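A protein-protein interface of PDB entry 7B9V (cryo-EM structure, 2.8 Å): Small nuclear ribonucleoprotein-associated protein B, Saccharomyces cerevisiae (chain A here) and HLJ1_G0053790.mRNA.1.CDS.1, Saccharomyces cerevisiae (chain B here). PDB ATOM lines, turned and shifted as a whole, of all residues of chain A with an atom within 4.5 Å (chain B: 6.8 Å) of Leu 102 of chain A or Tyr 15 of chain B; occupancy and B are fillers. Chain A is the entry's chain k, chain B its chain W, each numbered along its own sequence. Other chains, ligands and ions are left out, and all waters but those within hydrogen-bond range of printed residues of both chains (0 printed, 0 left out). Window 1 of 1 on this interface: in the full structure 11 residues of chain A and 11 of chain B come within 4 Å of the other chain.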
ATOM      1  N   LYS A  19      -9.301  25.473 -10.545  1.00  0.00           N
ATOM      2  CA  LYS A  19     -10.226  25.353  -9.429  1.00  0.00           C
ATOM      3  C   LYS A  19      -9.469  24.960  -8.170  1.00  0.00           C
ATOM      4  O   LYS A  19      -8.875  23.876  -8.089  1.00  0.00           O
ATOM      5  CB  LYS A  19     -11.344  24.357  -9.750  1.00  0.00           C
ATOM      6  CG  LYS A  19     -12.397  24.256  -8.658  1.00  0.00           C
ATOM      7  CD  LYS A  19     -13.771  23.876  -9.202  1.00  0.00           C
ATOM      8  CE  LYS A  19     -14.305  24.948 -10.156  1.00  0.00           C
ATOM      9  NZ  LYS A  19     -15.740  24.728 -10.497  1.00  0.00           N
ATOM     10  N   ASP A  99      -9.034  20.831  -9.973  1.00  0.00           N
ATOM     11  CA  ASP A  99      -8.650  20.515 -11.358  1.00  0.00           C
ATOM     12  C   ASP A  99      -8.381  21.778 -12.185  1.00  0.00           C
ATOM     13  O   ASP A  99      -8.572  22.912 -11.729  1.00  0.00           O
ATOM     14  CB  ASP A  99      -9.609  19.539 -12.094  1.00  0.00           C
ATOM     15  CG  ASP A  99     -11.054  19.994 -12.199  1.00  0.00           C
ATOM     16  OD1 ASP A  99     -11.391  21.203 -12.132  1.00  0.00           O
ATOM     17  OD2 ASP A  99     -11.884  19.084 -12.361  1.00  0.00           O
ATOM     18  N   LYS A 100      -7.882  21.535 -13.401  1.00  0.00           N
ATOM     19  CA  LYS A 100      -7.338  22.513 -14.333  1.00  0.00           C
ATOM     20  C   LYS A 100      -8.403  23.368 -15.043  1.00  0.00           C
ATOM     21  O   LYS A 100      -9.606  23.183 -14.836  1.00  0.00           O
ATOM     22  CB  LYS A 100      -6.510  21.708 -15.341  1.00  0.00           C
ATOM     23  CG  LYS A 100      -7.295  20.767 -16.224  1.00  0.00           C
ATOM     24  CD  LYS A 100      -6.368  20.032 -17.175  1.00  0.00           C
ATOM     25  CE  LYS A 100      -7.142  19.119 -18.100  1.00  0.00           C
ATOM     26  NZ  LYS A 100      -6.257  18.344 -19.008  1.00  0.00           N
ATOM     27  N   PRO A 101      -7.986  24.427 -15.919  1.00  0.00           N
ATOM     28  CA  PRO A 101      -8.997  25.215 -16.653  1.00  0.00           C
ATOM     29  C   PRO A 101      -9.623  24.440 -17.809  1.00  0.00           C
ATOM     30  O   PRO A 101      -9.021  24.282 -18.880  1.00  0.00           O
ATOM     31  CB  PRO A 101      -8.259  26.481 -17.125  1.00  0.00           C
ATOM     32  CG  PRO A 101      -7.061  26.562 -16.325  1.00  0.00           C
ATOM     33  CD  PRO A 101      -6.700  25.133 -16.092  1.00  0.00           C
ATOM     34  N   LEU A 102     -10.808  23.890 -17.573  1.00  0.00           N
ATOM     35  CA  LEU A 102     -11.546  23.165 -18.603  1.00  0.00           C
ATOM     36  C   LEU A 102     -12.077  24.110 -19.690  1.00  0.00           C
ATOM     37  O   LEU A 102     -12.152  25.330 -19.524  1.00  0.00           O
ATOM     38  CB  LEU A 102     -12.671  22.379 -17.927  1.00  0.00           C
ATOM     39  CG  LEU A 102     -12.401  20.941 -17.432  1.00  0.00           C
ATOM     40  CD1 LEU A 102     -11.183  20.735 -16.536  1.00  0.00           C
ATOM     41  CD2 LEU A 102     -13.617  20.494 -16.645  1.00  0.00           C
ATOM     42  N   LEU A 103     -12.408  23.526 -20.839  1.00  0.00           N
ATOM     43  CA  LEU A 103     -13.074  24.262 -21.911  1.00  0.00           C
ATOM     44  C   LEU A 103     -14.495  24.687 -21.524  1.00  0.00           C
ATOM     45  O   LEU A 103     -15.189  23.994 -20.782  1.00  0.00           O
ATOM     46  CB  LEU A 103     -13.083  23.360 -23.160  1.00  0.00           C
ATOM     47  CG  LEU A 103     -11.871  23.231 -24.121  1.00  0.00           C
ATOM     48  CD1 LEU A 103     -10.568  22.683 -23.513  1.00  0.00           C
ATOM     49  CD2 LEU A 103     -12.235  22.359 -25.323  1.00  0.00           C
ATOM     50  N   SER A 104     -14.936  25.843 -22.035  1.00  0.00           N
ATOM     51  CA  SER A 104     -16.339  26.210 -21.856  1.00  0.00           C
ATOM     52  C   SER A 104     -17.223  25.348 -22.737  1.00  0.00           C
ATOM     53  O   SER A 104     -16.786  24.860 -23.779  1.00  0.00           O
ATOM     54  CB  SER A 104     -16.562  27.685 -22.203  1.00  0.00           C
ATOM     55  OG  SER A 104     -16.346  27.927 -23.589  1.00  0.00           O
ATOM     56  N   LYS A 105     -18.453  25.083 -22.271  1.00  0.00           N
ATOM     57  CA  LYS A 105     -19.396  24.304 -23.080  1.00  0.00           C
ATOM     58  C   LYS A 105     -19.753  24.973 -24.407  1.00  0.00           C
ATOM     59  O   LYS A 105     -20.083  24.289 -25.384  1.00  0.00           O
ATOM     60  CB  LYS A 105     -20.633  24.004 -22.250  1.00  0.00           C
ATOM     61  CG  LYS A 105     -21.584  25.089 -21.913  1.00  0.00           C
ATOM     62  CD  LYS A 105     -22.495  24.536 -20.837  1.00  0.00           C
ATOM     63  CE  LYS A 105     -23.639  25.463 -20.625  1.00  0.00           C
ATOM     64  NZ  LYS A 105     -23.314  26.540 -19.670  1.00  0.00           N
ATOM     65  N   GLN B  13     -14.552  17.015 -21.715  1.00  0.00           N
ATOM     66  CA  GLN B  13     -15.106  17.319 -20.408  1.00  0.00           C
ATOM     67  C   GLN B  13     -15.194  18.816 -20.189  1.00  0.00           C
ATOM     68  O   GLN B  13     -14.412  19.602 -20.733  1.00  0.00           O
ATOM     69  CB  GLN B  13     -14.274  16.652 -19.311  1.00  0.00           C
ATOM     70  CG  GLN B  13     -12.903  17.242 -19.105  1.00  0.00           C
ATOM     71  CD  GLN B  13     -11.974  16.276 -18.418  1.00  0.00           C
ATOM     72  OE1 GLN B  13     -11.544  16.515 -17.299  1.00  0.00           O
ATOM     73  NE2 GLN B  13     -11.684  15.168 -19.076  1.00  0.00           N
ATOM     74  N   TYR B  14     -16.220  19.190 -19.418  1.00  0.00           N
ATOM     75  CA  TYR B  14     -16.577  20.581 -19.172  1.00  0.00           C
ATOM     76  C   TYR B  14     -17.509  20.661 -17.970  1.00  0.00           C
ATOM     77  O   TYR B  14     -18.033  19.652 -17.487  1.00  0.00           O
ATOM     78  CB  TYR B  14     -17.208  21.192 -20.438  1.00  0.00           C
ATOM     79  CG  TYR B  14     -18.374  20.428 -21.078  1.00  0.00           C
ATOM     80  CD1 TYR B  14     -18.163  19.333 -21.927  1.00  0.00           C
ATOM     81  CD2 TYR B  14     -19.667  20.909 -20.973  1.00  0.00           C
ATOM     82  CE1 TYR B  14     -19.224  18.649 -22.480  1.00  0.00           C
ATOM     83  CE2 TYR B  14     -20.717  20.284 -21.630  1.00  0.00           C
ATOM     84  CZ  TYR B  14     -20.498  19.142 -22.344  1.00  0.00           C
ATOM     85  OH  TYR B  14     -21.547  18.522 -22.985  1.00  0.00           O
ATOM     86  N   TYR B  15     -17.689  21.877 -17.481  1.00  0.00           N
ATOM     87  CA  TYR B  15     -18.631  22.175 -16.410  1.00  0.00           C
ATOM     88  C   TYR B  15     -20.006  22.521 -16.985  1.00  0.00           C
ATOM     89  O   TYR B  15     -20.107  23.201 -18.006  1.00  0.00           O
ATOM     90  CB  TYR B  15     -18.075  23.315 -15.552  1.00  0.00           C
ATOM     91  CG  TYR B  15     -16.957  22.877 -14.619  1.00  0.00           C
ATOM     92  CD1 TYR B  15     -17.239  22.080 -13.519  1.00  0.00           C
ATOM     93  CD2 TYR B  15     -15.629  23.256 -14.838  1.00  0.00           C
ATOM     94  CE1 TYR B  15     -16.235  21.649 -12.666  1.00  0.00           C
ATOM     95  CE2 TYR B  15     -14.612  22.835 -13.976  1.00  0.00           C
ATOM     96  CZ  TYR B  15     -14.931  22.024 -12.895  1.00  0.00           C
ATOM     97  OH  TYR B  15     -13.964  21.600 -12.015  1.00  0.00           O
ATOM     98  N   VAL B  16     -21.073  22.042 -16.322  1.00  0.00           N
ATOM     99  CA  VAL B  16     -22.467  22.253 -16.732  1.00  0.00           C
ATOM    100  C   VAL B  16     -23.360  22.681 -15.571  1.00  0.00           C
ATOM    101  O   VAL B  16     -23.169  22.257 -14.425  1.00  0.00           O
ATOM    102  CB  VAL B  16     -23.119  21.026 -17.405  1.00  0.00           C
ATOM    103  CG1 VAL B  16     -22.542  20.753 -18.698  1.00  0.00           C
ATOM    104  CG2 VAL B  16     -22.878  19.778 -16.568  1.00  0.00           C
ATOM    105  N   ASP B  17     -24.306  23.576 -15.869  1.00  0.00           N
ATOM    106  CA  ASP B  17     -25.145  24.248 -14.888  1.00  0.00           C
ATOM    107  C   ASP B  17     -26.422  23.489 -14.499  1.00  0.00           C
ATOM    108  O   ASP B  17     -27.132  23.987 -13.616  1.00  0.00           O
ATOM    109  CB  ASP B  17     -25.536  25.686 -15.298  1.00  0.00           C
ATOM    110  CG  ASP B  17     -25.313  26.014 -16.762  1.00  0.00           C
ATOM    111  OD1 ASP B  17     -24.959  25.115 -17.557  1.00  0.00           O
ATOM    112  OD2 ASP B  17     -25.442  27.207 -17.100  1.00  0.00           O
ATOM    113  N   ASN B  24     -21.757  27.012 -12.942  1.00  0.00           N
ATOM    114  CA  ASN B  24     -21.207  25.809 -13.565  1.00  0.00           C
ATOM    115  C   ASN B  24     -20.333  25.025 -12.579  1.00  0.00           C
ATOM    116  O   ASN B  24     -19.103  25.069 -12.622  1.00  0.00           O
ATOM    117  CB  ASN B  24     -20.417  26.207 -14.805  1.00  0.00           C
ATOM    118  CG  ASN B  24     -21.268  26.975 -15.818  1.00  0.00           C
ATOM    119  OD1 ASN B  24     -22.233  26.452 -16.353  1.00  0.00           O
ATOM    120  ND2 ASN B  24     -20.913  28.231 -16.049  1.00  0.00           N
ATOM    121  N   VAL B  25     -20.974  24.294 -11.661  1.00  0.00           N
ATOM    122  CA  VAL B  25     -20.264  23.692 -10.530  1.00  0.00           C
ATOM    123  C   VAL B  25     -20.247  22.164 -10.572  1.00  0.00           C
ATOM    124  O   VAL B  25     -19.713  21.540  -9.644  1.00  0.00           O
ATOM    125  CB  VAL B  25     -20.785  24.201  -9.169  1.00  0.00           C
ATOM    126  CG1 VAL B  25     -20.628  25.713  -9.083  1.00  0.00           C
ATOM    127  CG2 VAL B  25     -22.225  23.810  -8.959  1.00  0.00           C
ATOM    128  N   ASP B  26     -20.796  21.550 -11.620  1.00  0.00           N
ATOM    129  CA  ASP B  26     -20.831  20.105 -11.831  1.00  0.00           C
ATOM    130  C   ASP B  26     -20.184  19.772 -13.170  1.00  0.00           C
ATOM    131  O   ASP B  26     -20.435  20.445 -14.172  1.00  0.00           O
ATOM    132  CB  ASP B  26     -22.265  19.542 -11.801  1.00  0.00           C
ATOM    133  CG  ASP B  26     -22.983  19.810 -10.490  1.00  0.00           C
ATOM    134  OD1 ASP B  26     -23.617  20.878 -10.368  1.00  0.00           O
ATOM    135  OD2 ASP B  26     -22.969  18.925  -9.606  1.00  0.00           O
ATOM    136  N   LYS B  27     -19.341  18.739 -13.176  1.00  0.00           N
ATOM    137  CA  LYS B  27     -18.445  18.423 -14.281  1.00  0.00           C
ATOM    138  C   LYS B  27     -18.859  17.125 -14.956  1.00  0.00           C
ATOM    139  O   LYS B  27     -18.977  16.080 -14.300  1.00  0.00           O
ATOM    140  CB  LYS B  27     -17.022  18.256 -13.756  1.00  0.00           C
ATOM    141  CG  LYS B  27     -15.962  17.903 -14.774  1.00  0.00           C
ATOM    142  CD  LYS B  27     -14.623  17.919 -14.077  1.00  0.00           C
ATOM    143  CE  LYS B  27     -13.628  17.001 -14.738  1.00  0.00           C
ATOM    144  NZ  LYS B  27     -12.505  16.719 -13.806  1.00  0.00           N
ATOM    145  N   CYS B  28     -19.023  17.185 -16.269  1.00  0.00           N
ATOM    146  CA  CYS B  28     -19.400  16.047 -17.090  1.00  0.00           C
ATOM    147  C   CYS B  28     -18.205  15.478 -17.851  1.00  0.00           C
ATOM    148  O   CYS B  28     -17.373  16.228 -18.357  1.00  0.00           O
ATOM    149  CB  CYS B  28     -20.544  16.435 -18.027  1.00  0.00           C
ATOM    150  SG  CYS B  28     -20.152  17.640 -19.258  1.00  0.00           S
ATOM    151  N   THR B  51     -10.786  10.924 -14.898  1.00  0.00           N
ATOM    152  CA  THR B  51     -10.519  12.186 -14.183  1.00  0.00           C
ATOM    153  C   THR B  51     -11.326  12.326 -12.890  1.00  0.00           C
ATOM    154  O   THR B  51     -12.432  11.791 -12.749  1.00  0.00           O
ATOM    155  CB  THR B  51     -10.757  13.393 -15.106  1.00  0.00           C
ATOM    156  OG1 THR B  51     -10.496  14.611 -14.405  1.00  0.00           O
ATOM    157  CG2 THR B  51     -12.147  13.408 -15.612  1.00  0.00           C
ATOM    158  N   PRO B  53     -12.493  15.356  -9.739  1.00  0.00           N
ATOM    159  CA  PRO B  53     -13.800  14.715  -9.644  1.00  0.00           C
ATOM    160  C   PRO B  53     -14.550  14.663 -10.975  1.00  0.00           C
ATOM    161  O   PRO B  53     -14.281  15.441 -11.883  1.00  0.00           O
ATOM    162  CB  PRO B  53     -14.545  15.589  -8.621  1.00  0.00           C
ATOM    163  CG  PRO B  53     -14.066  16.960  -8.934  1.00  0.00           C
ATOM    164  CD  PRO B  53     -12.569  16.741  -9.252  1.00  0.00           C
ATOM    165  N   HIS B  55     -18.719  14.346 -12.035  1.00  0.00           N
ATOM    166  CA  HIS B  55     -20.041  14.396 -11.441  1.00  0.00           C
ATOM    167  C   HIS B  55     -21.057  13.685 -12.323  1.00  0.00           C
ATOM    168  O   HIS B  55     -21.894  12.940 -11.823  1.00  0.00           O
ATOM    169  CB  HIS B  55     -20.408  15.844 -11.164  1.00  0.00           C
ATOM    170  CG  HIS B  55     -19.453  16.497 -10.204  1.00  0.00           C
ATOM    171  ND1 HIS B  55     -18.477  17.380 -10.628  1.00  0.00           N
ATOM    172  CD2 HIS B  55     -19.251  16.327  -8.873  1.00  0.00           C
ATOM    173  CE1 HIS B  55     -17.759  17.761  -9.596  1.00  0.00           C
ATOM    174  NE2 HIS B  55     -18.206  17.135  -8.514  1.00  0.00           N
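The side-chain carboxylate (OD1) of Asp 17 of chain B lies within salt-bridge range of the side-chain amino group (NZ) of Lys 105 of chain A. The side-chain carboxylate of Asp 99 of chain A lies within salt-bridge range of the side-chain amino group of Lys 27 of chain B (2.8 Å). The side-chain carboxylate of Asp 99 of chain A sits at hydrogen-bond distance from the side-chain hydroxyl of Tyr 15 of chain B. OD1 of Asn 24 of chain B sits at hydrogen-bond distance from NZ of Lys 105 of chain A (3.5 Å).
The backbone carbonyl oxygen (O) of Lys 27 of chain B lies within hydrogen-bond range of the backbone NH (N) of His 55 of chain B, 2.9 Å away. The backbone carbonyl oxygen of Asp 99 of chain A sits at hydrogen-bond distance from the backbone NH of Lys 19 of chain A (2.9 Å). The side-chain amino group of Lys 27 of chain B lies within hydrogen-bond range of the side-chain hydroxyl of Thr 51 of chain B (3.0 Å). The backbone carbonyl oxygen of Pro 53 of chain B is in hydrogen-bond range of the side-chain amino group of Lys 27 of chain B (2.9 Å). OD1 of Asn 24 of chain B sits close to OD1 of Asp 17 of chain B (3.3 Å). The backbone NH (N) of Cys 28 of chain B sits at hydrogen-bond distance from the backbone carbonyl oxygen (O) of Tyr 14 of chain B.
OH of Tyr 15 of chain B touches CD of Lys 19 of chain A (3.6 Å). NZ of Lys 19 of chain A touches O of Asn 24 of chain B, 3.99 Å away. CD of Pro 53 of chain B touches OD2 of Asp 99 of chain A, 3.95 Å away. Tyr 14 of chain B touches Leu 102 of chain A. CD2 of Leu 102 of chain A touches CE2 of Tyr 15 of chain B, at 3.7 Å. Lys 27 of chain B touches Leu 102 of chain A. Tyr 14 of chain B touches Leu 103 of chain A. Lys 105 of chain A touches Tyr 14 of chain B (CB to CD2, 3.5 Å). Tyr 15 of chain B touches Lys 105 of chain A (O to CD, 3.9 Å).
Leu 102 of chain A touches just these residues of chain B: Tyr 14 (3.9 Å), Tyr 15 (3.7 Å) and Lys 27 (3.8 Å). Printed residues of chain A within 4 Å of Tyr 15 of chain B: Lys 19, Asp 99, Leu 102 and Lys 105. Of the printed residues of chain A, Tyr 14 of chain B touches Leu 102 (3.9 Å), Leu 103 (3.5 Å) and Lys 105 (3.5 Å). Printed residues of chain B within 4 Å of Lys 19 of chain A: Tyr 15 and Asn 24. Of the printed residues of chain B, Asp 99 of chain A touches Tyr 15, Lys 27 and Pro 53. Of the printed residues of chain A, Pro 53 of chain B touches Asp 99 (3.95 Å). Printed residues of chain B within 4 Å of Leu 103 of chain A: Tyr 14. Gln 13 of chain B touches none of the printed residues of chain A. The nearest printed residue of chain A that does not touch Tyr 15 of chain B is Leu 103 of chain A (4.7 Å). The nearest printed residue of chain B that does not touch Asp 99 of chain A is Thr 51 of chain B (5.1 Å).
Hydrophobic or aromatic side chains of chain A that line the printed part of chain B: Leu 102. Of the 13 printed residues of chain B, 6 touch a printed residue of chain A. Hydrophobic or aromatic side chains of chain B within 4 Å of the printed part of chain A: Tyr 14, Tyr 15 and Pro 53. Along chain B the printed residues that touch a printed residue of chain A span positions 14 to 53. Among the printed residues, Asp or Glu carboxylates within 4 Å of a Lys or Arg side-chain nitrogen of the other chain: Asp 99 of chain A with Lys 27 of chain B (2.8 Å) and Lys 105 of chain A with Asp 17 of chain B (3.0 Å).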
